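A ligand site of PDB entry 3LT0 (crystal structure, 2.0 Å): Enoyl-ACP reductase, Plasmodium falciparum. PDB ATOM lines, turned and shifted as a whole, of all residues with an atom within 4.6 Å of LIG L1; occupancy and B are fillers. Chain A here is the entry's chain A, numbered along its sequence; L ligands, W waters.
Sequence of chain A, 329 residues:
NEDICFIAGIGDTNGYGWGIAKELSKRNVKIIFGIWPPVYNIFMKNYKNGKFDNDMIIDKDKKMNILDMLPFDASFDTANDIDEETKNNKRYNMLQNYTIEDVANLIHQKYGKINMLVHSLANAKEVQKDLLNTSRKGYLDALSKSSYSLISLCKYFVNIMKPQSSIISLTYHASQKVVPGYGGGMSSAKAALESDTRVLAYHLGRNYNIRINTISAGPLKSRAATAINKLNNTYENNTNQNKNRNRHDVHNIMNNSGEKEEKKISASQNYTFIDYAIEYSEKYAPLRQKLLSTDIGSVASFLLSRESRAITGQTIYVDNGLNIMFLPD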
ATOM      1  N   GLY A   9       0.372  23.424   8.853  1.00  0.00           N
ATOM      2  CA  GLY A   9      -0.708  22.408   8.906  1.00  0.00           C
ATOM      3  C   GLY A   9      -1.010  21.803  10.267  1.00  0.00           C
ATOM      4  O   GLY A   9      -1.167  20.599  10.391  1.00  0.00           O
ATOM      5  N   ILE A  10      -1.071  22.625  11.298  1.00  0.00           N
ATOM      6  CA  ILE A  10      -1.503  22.202  12.625  1.00  0.00           C
ATOM      7  C   ILE A  10      -2.865  22.850  12.887  1.00  0.00           C
ATOM      8  O   ILE A  10      -3.022  24.072  12.737  1.00  0.00           O
ATOM      9  CB  ILE A  10      -0.441  22.522  13.698  1.00  0.00           C
ATOM     10  CG1 ILE A  10       0.695  21.486  13.587  1.00  0.00           C
ATOM     11  CG2 ILE A  10      -1.064  22.452  15.108  1.00  0.00           C
ATOM     12  CD1 ILE A  10       1.876  21.671  14.484  1.00  0.00           C
ATOM     13  N   GLY A  11      -3.871  22.035  13.217  1.00  0.00           N
ATOM     14  CA  GLY A  11      -5.209  22.524  13.555  1.00  0.00           C
ATOM     15  C   GLY A  11      -5.695  22.127  14.952  1.00  0.00           C
ATOM     16  O   GLY A  11      -6.668  22.707  15.467  1.00  0.00           O
ATOM     17  N   ASP A  12      -5.031  21.137  15.551  1.00  0.00           N
ATOM     18  CA  ASP A  12      -5.322  20.617  16.877  1.00  0.00           C
ATOM     19  C   ASP A  12      -4.197  19.635  17.214  1.00  0.00           C
ATOM     20  O   ASP A  12      -3.145  19.646  16.552  1.00  0.00           O
ATOM     21  CB  ASP A  12      -6.670  19.904  16.863  1.00  0.00           C
ATOM     22  CG  ASP A  12      -6.782  18.882  15.713  1.00  0.00           C
ATOM     23  OD1 ASP A  12      -7.755  18.951  14.934  1.00  0.00           O
ATOM     24  OD2 ASP A  12      -5.875  18.050  15.560  1.00  0.00           O
ATOM     25  N   GLY A  15      -3.378  15.330  14.897  1.00  0.00           N
ATOM     26  CA  GLY A  15      -2.869  15.012  13.561  1.00  0.00           C
ATOM     27  C   GLY A  15      -1.377  14.753  13.591  1.00  0.00           C
ATOM     28  O   GLY A  15      -0.756  14.740  14.665  1.00  0.00           O
ATOM     29  N   TYR A  16      -0.794  14.561  12.412  1.00  0.00           N
ATOM     30  CA  TYR A  16       0.648  14.316  12.340  1.00  0.00           C
ATOM     31  C   TYR A  16       1.500  15.554  12.628  1.00  0.00           C
ATOM     32  O   TYR A  16       2.605  15.411  13.117  1.00  0.00           O
ATOM     33  CB  TYR A  16       1.040  13.728  10.976  1.00  0.00           C
ATOM     34  CG  TYR A  16       0.717  12.242  10.883  1.00  0.00           C
ATOM     35  CD1 TYR A  16       1.257  11.355  11.817  1.00  0.00           C
ATOM     36  CD2 TYR A  16      -0.101  11.739   9.868  1.00  0.00           C
ATOM     37  CE1 TYR A  16       0.965   9.992  11.753  1.00  0.00           C
ATOM     38  CE2 TYR A  16      -0.365  10.363   9.774  1.00  0.00           C
ATOM     39  CZ  TYR A  16       0.183   9.508  10.722  1.00  0.00           C
ATOM     40  OH  TYR A  16      -0.045   8.154  10.673  1.00  0.00           O
ATOM     41  N   GLY A  17       0.980  16.736  12.353  1.00  0.00           N
ATOM     42  CA  GLY A  17       1.731  17.988  12.583  1.00  0.00           C
ATOM     43  C   GLY A  17       2.105  18.118  14.053  1.00  0.00           C
ATOM     44  O   GLY A  17       3.234  18.422  14.394  1.00  0.00           O
ATOM     45  N   TRP A  36      -4.206  27.153   9.553  1.00  0.00           N
ATOM     46  CA  TRP A  36      -5.209  27.534   8.560  1.00  0.00           C
ATOM     47  C   TRP A  36      -6.173  28.567   9.159  1.00  0.00           C
ATOM     48  O   TRP A  36      -6.727  28.338  10.247  1.00  0.00           O
ATOM     49  CB  TRP A  36      -5.935  26.276   8.106  1.00  0.00           C
ATOM     50  CG  TRP A  36      -6.762  26.425   6.878  1.00  0.00           C
ATOM     51  CD1 TRP A  36      -6.489  27.154   5.751  1.00  0.00           C
ATOM     52  CD2 TRP A  36      -8.009  25.759   6.627  1.00  0.00           C
ATOM     53  NE1 TRP A  36      -7.508  27.001   4.840  1.00  0.00           N
ATOM     54  CE2 TRP A  36      -8.441  26.138   5.347  1.00  0.00           C
ATOM     55  CE3 TRP A  36      -8.805  24.891   7.391  1.00  0.00           C
ATOM     56  CZ2 TRP A  36      -9.640  25.688   4.802  1.00  0.00           C
ATOM     57  CZ3 TRP A  36      -9.994  24.438   6.845  1.00  0.00           C
ATOM     58  CH2 TRP A  36     -10.393  24.829   5.561  1.00  0.00           C
ATOM     59  N   VAL A  39      -9.468  28.008  11.223  1.00  0.00           N
ATOM     60  CA  VAL A  39      -9.378  27.362  12.538  1.00  0.00           C
ATOM     61  C   VAL A  39      -8.385  28.040  13.482  1.00  0.00           C
ATOM     62  O   VAL A  39      -8.104  27.518  14.582  1.00  0.00           O
ATOM     63  CB  VAL A  39      -9.066  25.818  12.450  1.00  0.00           C
ATOM     64  CG1 VAL A  39     -10.039  25.094  11.512  1.00  0.00           C
ATOM     65  CG2 VAL A  39      -7.614  25.552  12.056  1.00  0.00           C
ATOM     66  N   PHE A  72      -1.891  30.902   8.371  1.00  0.00           N
ATOM     67  CA  PHE A  72      -1.184  30.458   7.176  1.00  0.00           C
ATOM     68  C   PHE A  72      -2.173  29.753   6.257  1.00  0.00           C
ATOM     69  O   PHE A  72      -2.847  28.819   6.659  1.00  0.00           O
ATOM     70  CB  PHE A  72      -0.056  29.487   7.573  1.00  0.00           C
ATOM     71  CG  PHE A  72       0.645  28.849   6.392  1.00  0.00           C
ATOM     72  CD1 PHE A  72       1.655  29.533   5.699  1.00  0.00           C
ATOM     73  CD2 PHE A  72       0.275  27.569   5.942  1.00  0.00           C
ATOM     74  CE1 PHE A  72       2.287  28.944   4.584  1.00  0.00           C
ATOM     75  CE2 PHE A  72       0.897  26.983   4.828  1.00  0.00           C
ATOM     76  CZ  PHE A  72       1.901  27.682   4.152  1.00  0.00           C
ATOM     77  N   ASP A  73      -2.318  30.252   5.041  1.00  0.00           N
ATOM     78  CA  ASP A  73      -3.196  29.625   4.071  1.00  0.00           C
ATOM     79  C   ASP A  73      -2.399  29.300   2.791  1.00  0.00           C
ATOM     80  O   ASP A  73      -1.920  30.215   2.088  1.00  0.00           O
ATOM     81  CB  ASP A  73      -4.388  30.537   3.780  1.00  0.00           C
ATOM     82  CG  ASP A  73      -5.476  29.840   3.007  1.00  0.00           C
ATOM     83  OD1 ASP A  73      -5.201  28.860   2.305  1.00  0.00           O
ATOM     84  OD2 ASP A  73      -6.646  30.269   3.122  1.00  0.00           O
ATOM     85  N   ALA A  74      -2.256  28.003   2.517  1.00  0.00           N
ATOM     86  CA  ALA A  74      -1.445  27.476   1.402  1.00  0.00           C
ATOM     87  C   ALA A  74      -2.136  27.642   0.052  1.00  0.00           C
ATOM     88  O   ALA A  74      -1.591  27.286  -0.996  1.00  0.00           O
ATOM     89  CB  ALA A  74      -1.138  26.017   1.655  1.00  0.00           C
ATOM     90  N   SER A  75      -3.376  28.126   0.091  1.00  0.00           N
ATOM     91  CA  SER A  75      -4.129  28.492  -1.108  1.00  0.00           C
ATOM     92  C   SER A  75      -3.548  29.701  -1.836  1.00  0.00           C
ATOM     93  O   SER A  75      -3.793  29.872  -3.040  1.00  0.00           O
ATOM     94  CB  SER A  75      -5.569  28.854  -0.741  1.00  0.00           C
ATOM     95  OG  SER A  75      -6.229  27.795  -0.095  1.00  0.00           O
ATOM     96  N   SER A 120       2.574  19.737   6.310  1.00  0.00           N
ATOM     97  CA  SER A 120       1.714  18.704   6.892  1.00  0.00           C
ATOM     98  C   SER A 120       0.255  19.068   6.680  1.00  0.00           C
ATOM     99  O   SER A 120      -0.514  19.190   7.638  1.00  0.00           O
ATOM    100  CB  SER A 120       2.027  18.541   8.396  1.00  0.00           C
ATOM    101  OG  SER A 120       1.312  17.431   8.922  1.00  0.00           O
ATOM    102  N   LEU A 121      -0.112  19.290   5.433  1.00  0.00           N
ATOM    103  CA  LEU A 121      -1.443  19.761   5.114  1.00  0.00           C
ATOM    104  C   LEU A 121      -1.896  19.172   3.778  1.00  0.00           C
ATOM    105  O   LEU A 121      -1.047  18.825   2.894  1.00  0.00           O
ATOM    106  CB  LEU A 121      -1.500  21.310   5.055  1.00  0.00           C
ATOM    107  CG  LEU A 121      -0.675  22.017   3.961  1.00  0.00           C
ATOM    108  CD1 LEU A 121      -1.470  22.262   2.674  1.00  0.00           C
ATOM    109  CD2 LEU A 121      -0.023  23.354   4.467  1.00  0.00           C
ATOM    110  N   ALA A 122      -3.215  19.134   3.606  1.00  0.00           N
ATOM    111  CA  ALA A 122      -3.829  18.725   2.350  1.00  0.00           C
ATOM    112  C   ALA A 122      -5.253  19.217   2.367  1.00  0.00           C
ATOM    113  O   ALA A 122      -5.825  19.416   3.433  1.00  0.00           O
ATOM    114  CB  ALA A 122      -3.789  17.206   2.212  1.00  0.00           C
ATOM    115  N   ASN A 123      -5.838  19.381   1.194  1.00  0.00           N
ATOM    116  CA  ASN A 123      -7.264  19.701   1.129  1.00  0.00           C
ATOM    117  C   ASN A 123      -7.759  19.322  -0.261  1.00  0.00           C
ATOM    118  O   ASN A 123      -6.968  19.291  -1.205  1.00  0.00           O
ATOM    119  CB  ASN A 123      -7.505  21.187   1.447  1.00  0.00           C
ATOM    120  CG  ASN A 123      -8.851  21.447   2.171  1.00  0.00           C
ATOM    121  OD1 ASN A 123      -8.991  22.430   2.895  1.00  0.00           O
ATOM    122  ND2 ASN A 123      -9.820  20.565   1.961  1.00  0.00           N
ATOM    123  N   LYS A 145      -4.006  22.806  -3.432  1.00  0.00           N
ATOM    124  CA  LYS A 145      -3.840  22.846  -1.985  1.00  0.00           C
ATOM    125  C   LYS A 145      -2.864  21.833  -1.450  1.00  0.00           C
ATOM    126  O   LYS A 145      -2.185  22.106  -0.449  1.00  0.00           O
ATOM    127  CB  LYS A 145      -5.177  22.633  -1.262  1.00  0.00           C
ATOM    128  CG  LYS A 145      -6.293  23.614  -1.650  1.00  0.00           C
ATOM    129  CD  LYS A 145      -5.857  25.034  -1.767  1.00  0.00           C
ATOM    130  CE  LYS A 145      -7.013  25.863  -2.401  1.00  0.00           C
ATOM    131  NZ  LYS A 145      -8.338  25.620  -1.714  1.00  0.00           N
ATOM    132  N   LEU A 170       4.156  15.059   3.932  1.00  0.00           N
ATOM    133  CA  LEU A 170       3.510  13.779   4.250  1.00  0.00           C
ATOM    134  C   LEU A 170       2.670  13.327   3.034  1.00  0.00           C
ATOM    135  O   LEU A 170       1.960  14.126   2.420  1.00  0.00           O
ATOM    136  CB  LEU A 170       2.623  13.949   5.481  1.00  0.00           C
ATOM    137  CG  LEU A 170       3.358  14.216   6.806  1.00  0.00           C
ATOM    138  CD1 LEU A 170       2.387  14.727   7.851  1.00  0.00           C
ATOM    139  CD2 LEU A 170       3.979  12.930   7.326  1.00  0.00           C
ATOM    140  N   THR A 171       2.757  12.055   2.709  1.00  0.00           N
ATOM    141  CA  THR A 171       1.997  11.499   1.598  1.00  0.00           C
ATOM    142  C   THR A 171       1.262  10.227   2.072  1.00  0.00           C
ATOM    143  O   THR A 171       1.315   9.860   3.260  1.00  0.00           O
ATOM    144  CB  THR A 171       2.921  11.275   0.354  1.00  0.00           C
ATOM    145  OG1 THR A 171       2.141  10.895  -0.796  1.00  0.00           O
ATOM    146  CG2 THR A 171       3.975  10.172   0.675  1.00  0.00           C
ATOM    147  N   TYR A 172       0.580   9.559   1.138  1.00  0.00           N
ATOM    148  CA  TYR A 172      -0.136   8.329   1.462  1.00  0.00           C
ATOM    149  C   TYR A 172      -0.061   7.405   0.244  1.00  0.00           C
ATOM    150  O   TYR A 172      -0.054   7.891  -0.907  1.00  0.00           O
ATOM    151  CB  TYR A 172      -1.593   8.663   1.823  1.00  0.00           C
ATOM    152  CG  TYR A 172      -2.448   7.457   2.160  1.00  0.00           C
ATOM    153  CD1 TYR A 172      -2.080   6.576   3.185  1.00  0.00           C
ATOM    154  CD2 TYR A 172      -3.634   7.195   1.461  1.00  0.00           C
ATOM    155  CE1 TYR A 172      -2.839   5.467   3.490  1.00  0.00           C
ATOM    156  CE2 TYR A 172      -4.430   6.064   1.771  1.00  0.00           C
ATOM    157  CZ  TYR A 172      -4.011   5.222   2.786  1.00  0.00           C
ATOM    158  OH  TYR A 172      -4.741   4.107   3.101  1.00  0.00           O
ATOM    159  N   TYR A 182     -10.457   7.126  -1.337  1.00  0.00           N
ATOM    160  CA  TYR A 182      -9.502   8.257  -1.271  1.00  0.00           C
ATOM    161  C   TYR A 182      -9.720   9.090  -2.529  1.00  0.00           C
ATOM    162  O   TYR A 182      -8.952   9.010  -3.484  1.00  0.00           O
ATOM    163  CB  TYR A 182      -8.066   7.721  -1.170  1.00  0.00           C
ATOM    164  CG  TYR A 182      -7.030   8.728  -0.650  1.00  0.00           C
ATOM    165  CD1 TYR A 182      -7.032   9.143   0.681  1.00  0.00           C
ATOM    166  CD2 TYR A 182      -6.034   9.239  -1.506  1.00  0.00           C
ATOM    167  CE1 TYR A 182      -6.075  10.085   1.146  1.00  0.00           C
ATOM    168  CE2 TYR A 182      -5.075  10.147  -1.057  1.00  0.00           C
ATOM    169  CZ  TYR A 182      -5.100  10.554   0.257  1.00  0.00           C
ATOM    170  OH  TYR A 182      -4.131  11.417   0.704  1.00  0.00           O
ATOM    171  N   LYS A 190      -1.239  13.304  -4.308  1.00  0.00           N
ATOM    172  CA  LYS A 190      -0.153  12.601  -3.589  1.00  0.00           C
ATOM    173  C   LYS A 190       0.872  12.013  -4.584  1.00  0.00           C
ATOM    174  O   LYS A 190       2.069  12.008  -4.296  1.00  0.00           O
ATOM    175  CB  LYS A 190      -0.713  11.508  -2.658  1.00  0.00           C
ATOM    176  CG  LYS A 190      -1.504  12.030  -1.432  1.00  0.00           C
ATOM    177  CD  LYS A 190      -0.716  13.145  -0.652  1.00  0.00           C
ATOM    178  CE  LYS A 190      -1.418  13.427   0.691  1.00  0.00           C
ATOM    179  NZ  LYS A 190      -0.762  14.552   1.466  1.00  0.00           N
ATOM    180  N   ALA A 217       2.875   8.053   5.462  1.00  0.00           N
ATOM    181  CA  ALA A 217       2.340   7.587   6.761  1.00  0.00           C
ATOM    182  C   ALA A 217       1.190   6.595   6.632  1.00  0.00           C
ATOM    183  O   ALA A 217       0.425   6.642   5.662  1.00  0.00           O
ATOM    184  CB  ALA A 217       1.896   8.755   7.582  1.00  0.00           C
ATOM    185  N   GLY A 218       1.060   5.701   7.616  1.00  0.00           N
ATOM    186  CA  GLY A 218      -0.146   4.885   7.734  1.00  0.00           C
ATOM    187  C   GLY A 218      -1.278   5.690   8.352  1.00  0.00           C
ATOM    188  O   GLY A 218      -1.133   6.905   8.612  1.00  0.00           O
ATOM    189  N   PRO A 219      -2.435   5.026   8.572  1.00  0.00           N
ATOM    190  CA  PRO A 219      -3.641   5.750   8.995  1.00  0.00           C
ATOM    191  C   PRO A 219      -3.624   6.236  10.456  1.00  0.00           C
ATOM    192  O   PRO A 219      -3.178   5.514  11.367  1.00  0.00           O
ATOM    193  CB  PRO A 219      -4.756   4.741   8.755  1.00  0.00           C
ATOM    194  CG  PRO A 219      -4.042   3.348   8.932  1.00  0.00           C
ATOM    195  CD  PRO A 219      -2.667   3.579   8.356  1.00  0.00           C
ATOM    196  N   LEU A 220      -4.128   7.450  10.652  1.00  0.00           N
ATOM    197  CA  LEU A 220      -4.248   8.057  11.968  1.00  0.00           C
ATOM    198  C   LEU A 220      -5.574   8.781  12.011  1.00  0.00           C
ATOM    199  O   LEU A 220      -5.947   9.464  11.041  1.00  0.00           O
ATOM    200  CB  LEU A 220      -3.142   9.075  12.187  1.00  0.00           C
ATOM    201  CG  LEU A 220      -3.084   9.861  13.512  1.00  0.00           C
ATOM    202  CD1 LEU A 220      -2.481   8.969  14.616  1.00  0.00           C
ATOM    203  CD2 LEU A 220      -2.233  11.129  13.286  1.00  0.00           C
ATOM    204  N   SER A 222      -7.091  11.521  12.533  1.00  0.00           N
ATOM    205  CA  SER A 222      -6.952  12.971  12.642  1.00  0.00           C
ATOM    206  C   SER A 222      -8.282  13.624  12.240  1.00  0.00           C
ATOM    207  O   SER A 222      -9.200  12.924  11.783  1.00  0.00           O
ATOM    208  CB  SER A 222      -5.861  13.453  11.694  1.00  0.00           C
ATOM    209  OG  SER A 222      -6.249  13.131  10.358  1.00  0.00           O
ATOM    210  N   ARG A 223      -8.380  14.941  12.396  1.00  0.00           N
ATOM    211  CA  ARG A 223      -9.598  15.632  11.951  1.00  0.00           C
ATOM    212  C   ARG A 223      -9.853  15.399  10.471  1.00  0.00           C
ATOM    213  O   ARG A 223     -10.960  14.979  10.099  1.00  0.00           O
ATOM    214  CB  ARG A 223      -9.562  17.159  12.226  1.00  0.00           C
ATOM    215  CG  ARG A 223     -10.732  17.894  11.516  1.00  0.00           C
ATOM    216  CD  ARG A 223     -11.073  19.247  12.117  1.00  0.00           C
ATOM    217  NE  ARG A 223      -9.904  20.106  12.289  1.00  0.00           N
ATOM    218  CZ  ARG A 223      -9.904  21.245  12.967  1.00  0.00           C
ATOM    219  NH1 ARG A 223     -11.026  21.673  13.537  1.00  0.00           N
ATOM    220  NH2 ARG A 223      -8.781  21.959  13.085  1.00  0.00           N
ATOM    221  N   ALA A 224      -8.863  15.630   9.623  1.00  0.00           N
ATOM    222  CA  ALA A 224      -9.053  15.452   8.191  1.00  0.00           C
ATOM    223  C   ALA A 224      -9.477  14.031   7.808  1.00  0.00           C
ATOM    224  O   ALA A 224     -10.379  13.845   6.988  1.00  0.00           O
ATOM    225  CB  ALA A 224      -7.796  15.845   7.431  1.00  0.00           C
ATOM    226  N   ALA A 225      -8.835  13.037   8.409  1.00  0.00           N
ATOM    227  CA  ALA A 225      -9.159  11.639   8.119  1.00  0.00           C
ATOM    228  C   ALA A 225     -10.643  11.364   8.313  1.00  0.00           C
ATOM    229  O   ALA A 225     -11.234  10.548   7.602  1.00  0.00           O
ATOM    230  CB  ALA A 225      -8.319  10.719   8.981  1.00  0.00           C
ATOM    231  N   ILE A 274     -11.716   5.933   7.842  1.00  0.00           N
ATOM    232  CA  ILE A 274     -10.541   5.884   8.708  1.00  0.00           C
ATOM    233  C   ILE A 274     -10.609   4.775   9.746  1.00  0.00           C
ATOM    234  O   ILE A 274      -9.588   4.171  10.065  1.00  0.00           O
ATOM    235  CB  ILE A 274     -10.203   7.272   9.365  1.00  0.00           C
ATOM    236  CG1 ILE A 274      -8.790   7.243   9.970  1.00  0.00           C
ATOM    237  CG2 ILE A 274     -11.285   7.705  10.410  1.00  0.00           C
ATOM    238  CD1 ILE A 274      -7.693   6.993   8.974  1.00  0.00           C
HETATM  239  P1  LIG L   1      -4.985  17.107  10.163  1.00  0.00           P
HETATM  240  O1  LIG L   1      -6.367  17.663   9.903  1.00  0.00           O
HETATM  241  O2  LIG L   1      -4.456  16.948  11.572  1.00  0.00           O
HETATM  242  O3  LIG L   1      -3.921  17.982   9.332  1.00  0.00           O
HETATM  243  C1  LIG L   1      -4.306  18.633   8.114  1.00  0.00           C
HETATM  244  C2  LIG L   1      -4.203  20.142   8.327  1.00  0.00           C
HETATM  245  O4  LIG L   1      -4.073  20.842   7.082  1.00  0.00           O
HETATM  246  C3  LIG L   1      -5.420  20.722   9.029  1.00  0.00           C
HETATM  247  O5  LIG L   1      -5.038  21.193  10.318  1.00  0.00           O
HETATM  248  C4  LIG L   1      -5.868  21.894   8.173  1.00  0.00           C
HETATM  249  O6  LIG L   1      -6.122  23.043   8.966  1.00  0.00           O
HETATM  250  C5  LIG L   1      -4.686  22.117   7.244  1.00  0.00           C
HETATM  251  N1  LIG L   1      -5.133  22.729   5.965  1.00  0.00           N
HETATM  252  C6  LIG L   1      -6.145  22.345   5.174  1.00  0.00           C
HETATM  253  N2  LIG L   1      -6.236  23.182   4.101  1.00  0.00           N
HETATM  254  C7  LIG L   1      -5.268  24.106   4.253  1.00  0.00           C
HETATM  255  C8  LIG L   1      -4.819  25.282   3.456  1.00  0.00           C
HETATM  256  N3  LIG L   1      -5.434  25.622   2.295  1.00  0.00           N
HETATM  257  N4  LIG L   1      -3.771  26.005   3.923  1.00  0.00           N
HETATM  258  C9  LIG L   1      -3.169  25.654   5.066  1.00  0.00           C
HETATM  259  N5  LIG L   1      -3.559  24.598   5.798  1.00  0.00           N
HETATM  260  C10 LIG L   1      -4.580  23.812   5.422  1.00  0.00           C
HETATM  261  O7  LIG L   1      -4.893  15.674   9.428  1.00  0.00           O
HETATM  262  P2  LIG L   1      -3.484  14.920   9.222  1.00  0.00           P
HETATM  263  O8  LIG L   1      -3.792  13.459   9.003  1.00  0.00           O
HETATM  264  O9  LIG L   1      -2.563  15.334  10.338  1.00  0.00           O
HETATM  265  O10 LIG L   1      -2.924  15.533   7.845  1.00  0.00           O
HETATM  266  C11 LIG L   1      -1.553  15.930   7.759  1.00  0.00           C
HETATM  267  C12 LIG L   1      -0.902  15.343   6.511  1.00  0.00           C
HETATM  268  O11 LIG L   1      -0.632  13.943   6.695  1.00  0.00           O
HETATM  269  C13 LIG L   1      -1.787  15.464   5.281  1.00  0.00           C
HETATM  270  O12 LIG L   1      -0.999  15.939   4.189  1.00  0.00           O
HETATM  271  C14 LIG L   1      -2.237  14.057   5.000  1.00  0.00           C
HETATM  272  O13 LIG L   1      -2.422  13.851   3.593  1.00  0.00           O
HETATM  273  C15 LIG L   1      -1.091  13.234   5.543  1.00  0.00           C
HETATM  274  N6  LIG L   1      -1.485  11.850   5.853  1.00  0.00           N
HETATM  275  C16 LIG L   1      -2.409  11.587   6.785  1.00  0.00           C
HETATM  276  C17 LIG L   1      -2.777  10.267   7.083  1.00  0.00           C
HETATM  277  C18 LIG L   1      -3.807   9.987   8.125  1.00  0.00           C
HETATM  278  O14 LIG L   1      -4.276   8.860   8.203  1.00  0.00           O
HETATM  279  N7  LIG L   1      -4.197  10.954   8.947  1.00  0.00           N
HETATM  280  C19 LIG L   1      -2.146   9.102   6.353  1.00  0.00           C
HETATM  281  C20 LIG L   1      -1.172   9.532   5.369  1.00  0.00           C
HETATM  282  C21 LIG L   1      -0.888  10.878   5.163  1.00  0.00           C
HETATM  283  C1  LG2 L   2      -5.404  11.908   5.083  1.00  0.00           C
HETATM  284  C2  LG2 L   2      -4.655  11.199   4.145  1.00  0.00           C
HETATM  285  C3  LG2 L   2      -4.675   9.804   4.152  1.00  0.00           C
HETATM  286  C4  LG2 L   2      -5.468   9.111   5.079  1.00  0.00           C
HETATM  287  C5  LG2 L   2      -6.222   9.842   6.013  1.00  0.00           C
HETATM  288  C6  LG2 L   2      -6.189  11.247   6.024  1.00  0.00           C
HETATM  289  O1  LG2 L   2      -5.349  13.278   5.048  1.00  0.00           O
HETATM  290  C7  LG2 L   2      -6.250  13.986   4.257  1.00  0.00           C
HETATM  291  C8  LG2 L   2      -6.281  15.371   4.356  1.00  0.00           C
HETATM  292  C9  LG2 L   2      -7.168  16.133   3.596  1.00  0.00           C
HETATM  293  C10 LG2 L   2      -8.027  15.449   2.736  1.00  0.00           C
HETATM  294  C11 LG2 L   2      -8.017  14.063   2.607  1.00  0.00           C
HETATM  295  C12 LG2 L   2      -7.123  13.332   3.372  1.00  0.00           C
HETATM  296  C13 LG2 L   2      -5.479   7.630   5.079  1.00  0.00           C
HETATM  297  O2  LG2 L   2      -6.117   7.024   5.941  1.00  0.00           O
HETATM  298 CL1  LG2 L   2      -9.164  16.423   1.781  1.00  0.00          CL
HETATM  299 CL2  LG2 L   2      -5.174  16.211   5.480  1.00  0.00          CL
HETATM  300  O3  LG2 L   2      -3.906  11.882   3.223  1.00  0.00           O
HETATM  301  O   HOH W   1      -1.073  17.791  10.756  1.00  0.00           O
HETATM  302  O   HOH W   2      -6.799  19.558  12.011  1.00  0.00           O
HETATM  303  O   HOH W   3      -3.993  24.169  10.419  1.00  0.00           O
HETATM  304  O   HOH W   4      -8.209  25.166   1.080  1.00  0.00           O
HETATM  305  O   HOH W   5      -8.377  19.118   8.773  1.00  0.00           O
HETATM  306  O   HOH W   6       1.832  17.042   3.492  1.00  0.00           O
HETATM  307  O   HOH W   7      -8.356  21.937  10.361  1.00  0.00           O
HETATM  308  O   HOH W   8      -3.877  19.182  13.209  1.00  0.00           O
HETATM  309  O   HOH W   9      -6.126  16.302  13.588  1.00  0.00           O
HETATM  310  O   HOH W  10      -1.877  25.065   8.020  1.00  0.00           O
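O of Gly 11 lies within hydrogen-bond range of NH2 of Arg 223, at 3.3 Å. The backbone carbonyl oxygen (O) of Thr 171 sits at hydrogen-bond distance from the backbone NH (N) of Ala 217 (3.2 Å). The side-chain hydroxyl of Ser 75 lies within hydrogen-bond range of the side-chain carboxylate of Asp 73 (2.8 Å). The side-chain hydroxyl (OH) of Tyr 16 lies within hydrogen-bond range of the backbone carbonyl oxygen (O) of Gly 218, at 2.6 Å. The backbone NH (N) of Ala 225 is in hydrogen-bond range of the side-chain hydroxyl (OG) of Ser 222. NE of Arg 223 is in salt-bridge range of OD1 of Asp 12. O of Leu 170 lies within hydrogen-bond range of NZ of Lys 190 (2.9 Å). OG of Ser 75 sits close to NZ of Lys 145 (3.4 Å).
The side-chain hydroxyl (OG) of Ser 222 is in hydrogen-bond range of an oxygen (O8) of LIG L1 (2.8 Å). The backbone NH of Ala 224 is in hydrogen-bond range of an oxygen (O1) of LIG L1, at 3.2 Å. The backbone carbonyl oxygen of Leu 121 lies within hydrogen-bond range of an oxygen (O12) of LIG L1 (3.2 Å). The side-chain hydroxyl of Tyr 182 lies within hydrogen-bond range of an oxygen (O3) of LG2 L2, at 2.6 Å. N of Tyr 16 lies within hydrogen-bond range of O9 of LIG L1 (2.8 Å). An oxygen (O13) of LIG L1 is in hydrogen-bond range of the side-chain amino group (NZ) of Lys 190, 2.8 Å away. O of Leu 220 sits at hydrogen-bond distance from N7 of LIG L1 (3.1 Å). A nitrogen (N2) of LIG L1 lies close to the side-chain amide oxygen (OD1) of Asn 123, 3.1 Å away. OD1 of Asp 73 lies within hydrogen-bond range of N3 of LIG L1. N of Ala 74 is in hydrogen-bond range of N4 of LIG L1, at 2.9 Å. The side-chain hydroxyl of Ser 75 lies within hydrogen-bond range of a nitrogen (N3) of LIG L1 (3.3 Å). The backbone NH (N) of Gly 11 sits at hydrogen-bond distance from an oxygen (O5) of LIG L1 (3.2 Å). An oxygen (O14) of LIG L1 is in hydrogen-bond range of the backbone NH (N) of Leu 220 (2.8 Å).
O13 of LIG L1 sits at hydrogen-bond distance from O3 of LG2 L2, 2.5 Å away.
Water W9 lies within hydrogen-bond range of the side-chain carboxylate (OD2) of Asp 12 (2.6 Å), an oxygen (O2) of LIG L1 (2.7 Å), the backbone NH (N) of Arg 223 (2.9 Å) and the backbone NH (N) of Gly 15 (3.2 Å). Water W3 lies within hydrogen-bond range of O of Ile 10, O6 of LIG L1 and N of Trp 36. Water W7 lies within hydrogen-bond range of the guanidinium group of Arg 223 (2.8 Å) and an oxygen (O6) of LIG L1 (2.9 Å). Water W2 lies within hydrogen-bond range of O1 of LIG L1 (2.9 Å), OD1 of Asp 12 (3.1 Å) and NE of Arg 223 (3.2 Å). Water W4 lies within hydrogen-bond range of NZ of Lys 145 (2.8 Å), N3 of LIG L1 (3.1 Å), OD1 of Asn 123 (3.4 Å) and OG of Ser 75 (3.5 Å). Water W6 lies within hydrogen-bond range of N of Leu 170 (3.1 Å), O12 of LIG L1 (3.1 Å) and O of Leu 121 (3.4 Å).
Residues that only touch LIG L1: Thr 171, Gly 15, Pro 219, Gly 218, Ala 217, Leu 170, Trp 36, Ala 122, Ser 120, Phe 72, Tyr 172, Gly 9, Ile 10, Ile 274 and Arg 223. Hydrophobic or aromatic side chains within 4 Å of LIG L1: Tyr 16, Trp 36, Ala 74, Leu 121, Ala 122, Leu 170, Tyr 172, Ala 217, Leu 220, Ala 224 and Ile 274. The nearest printed residue that does not touch LIG L1 is Lys 145 (4.1 Å).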
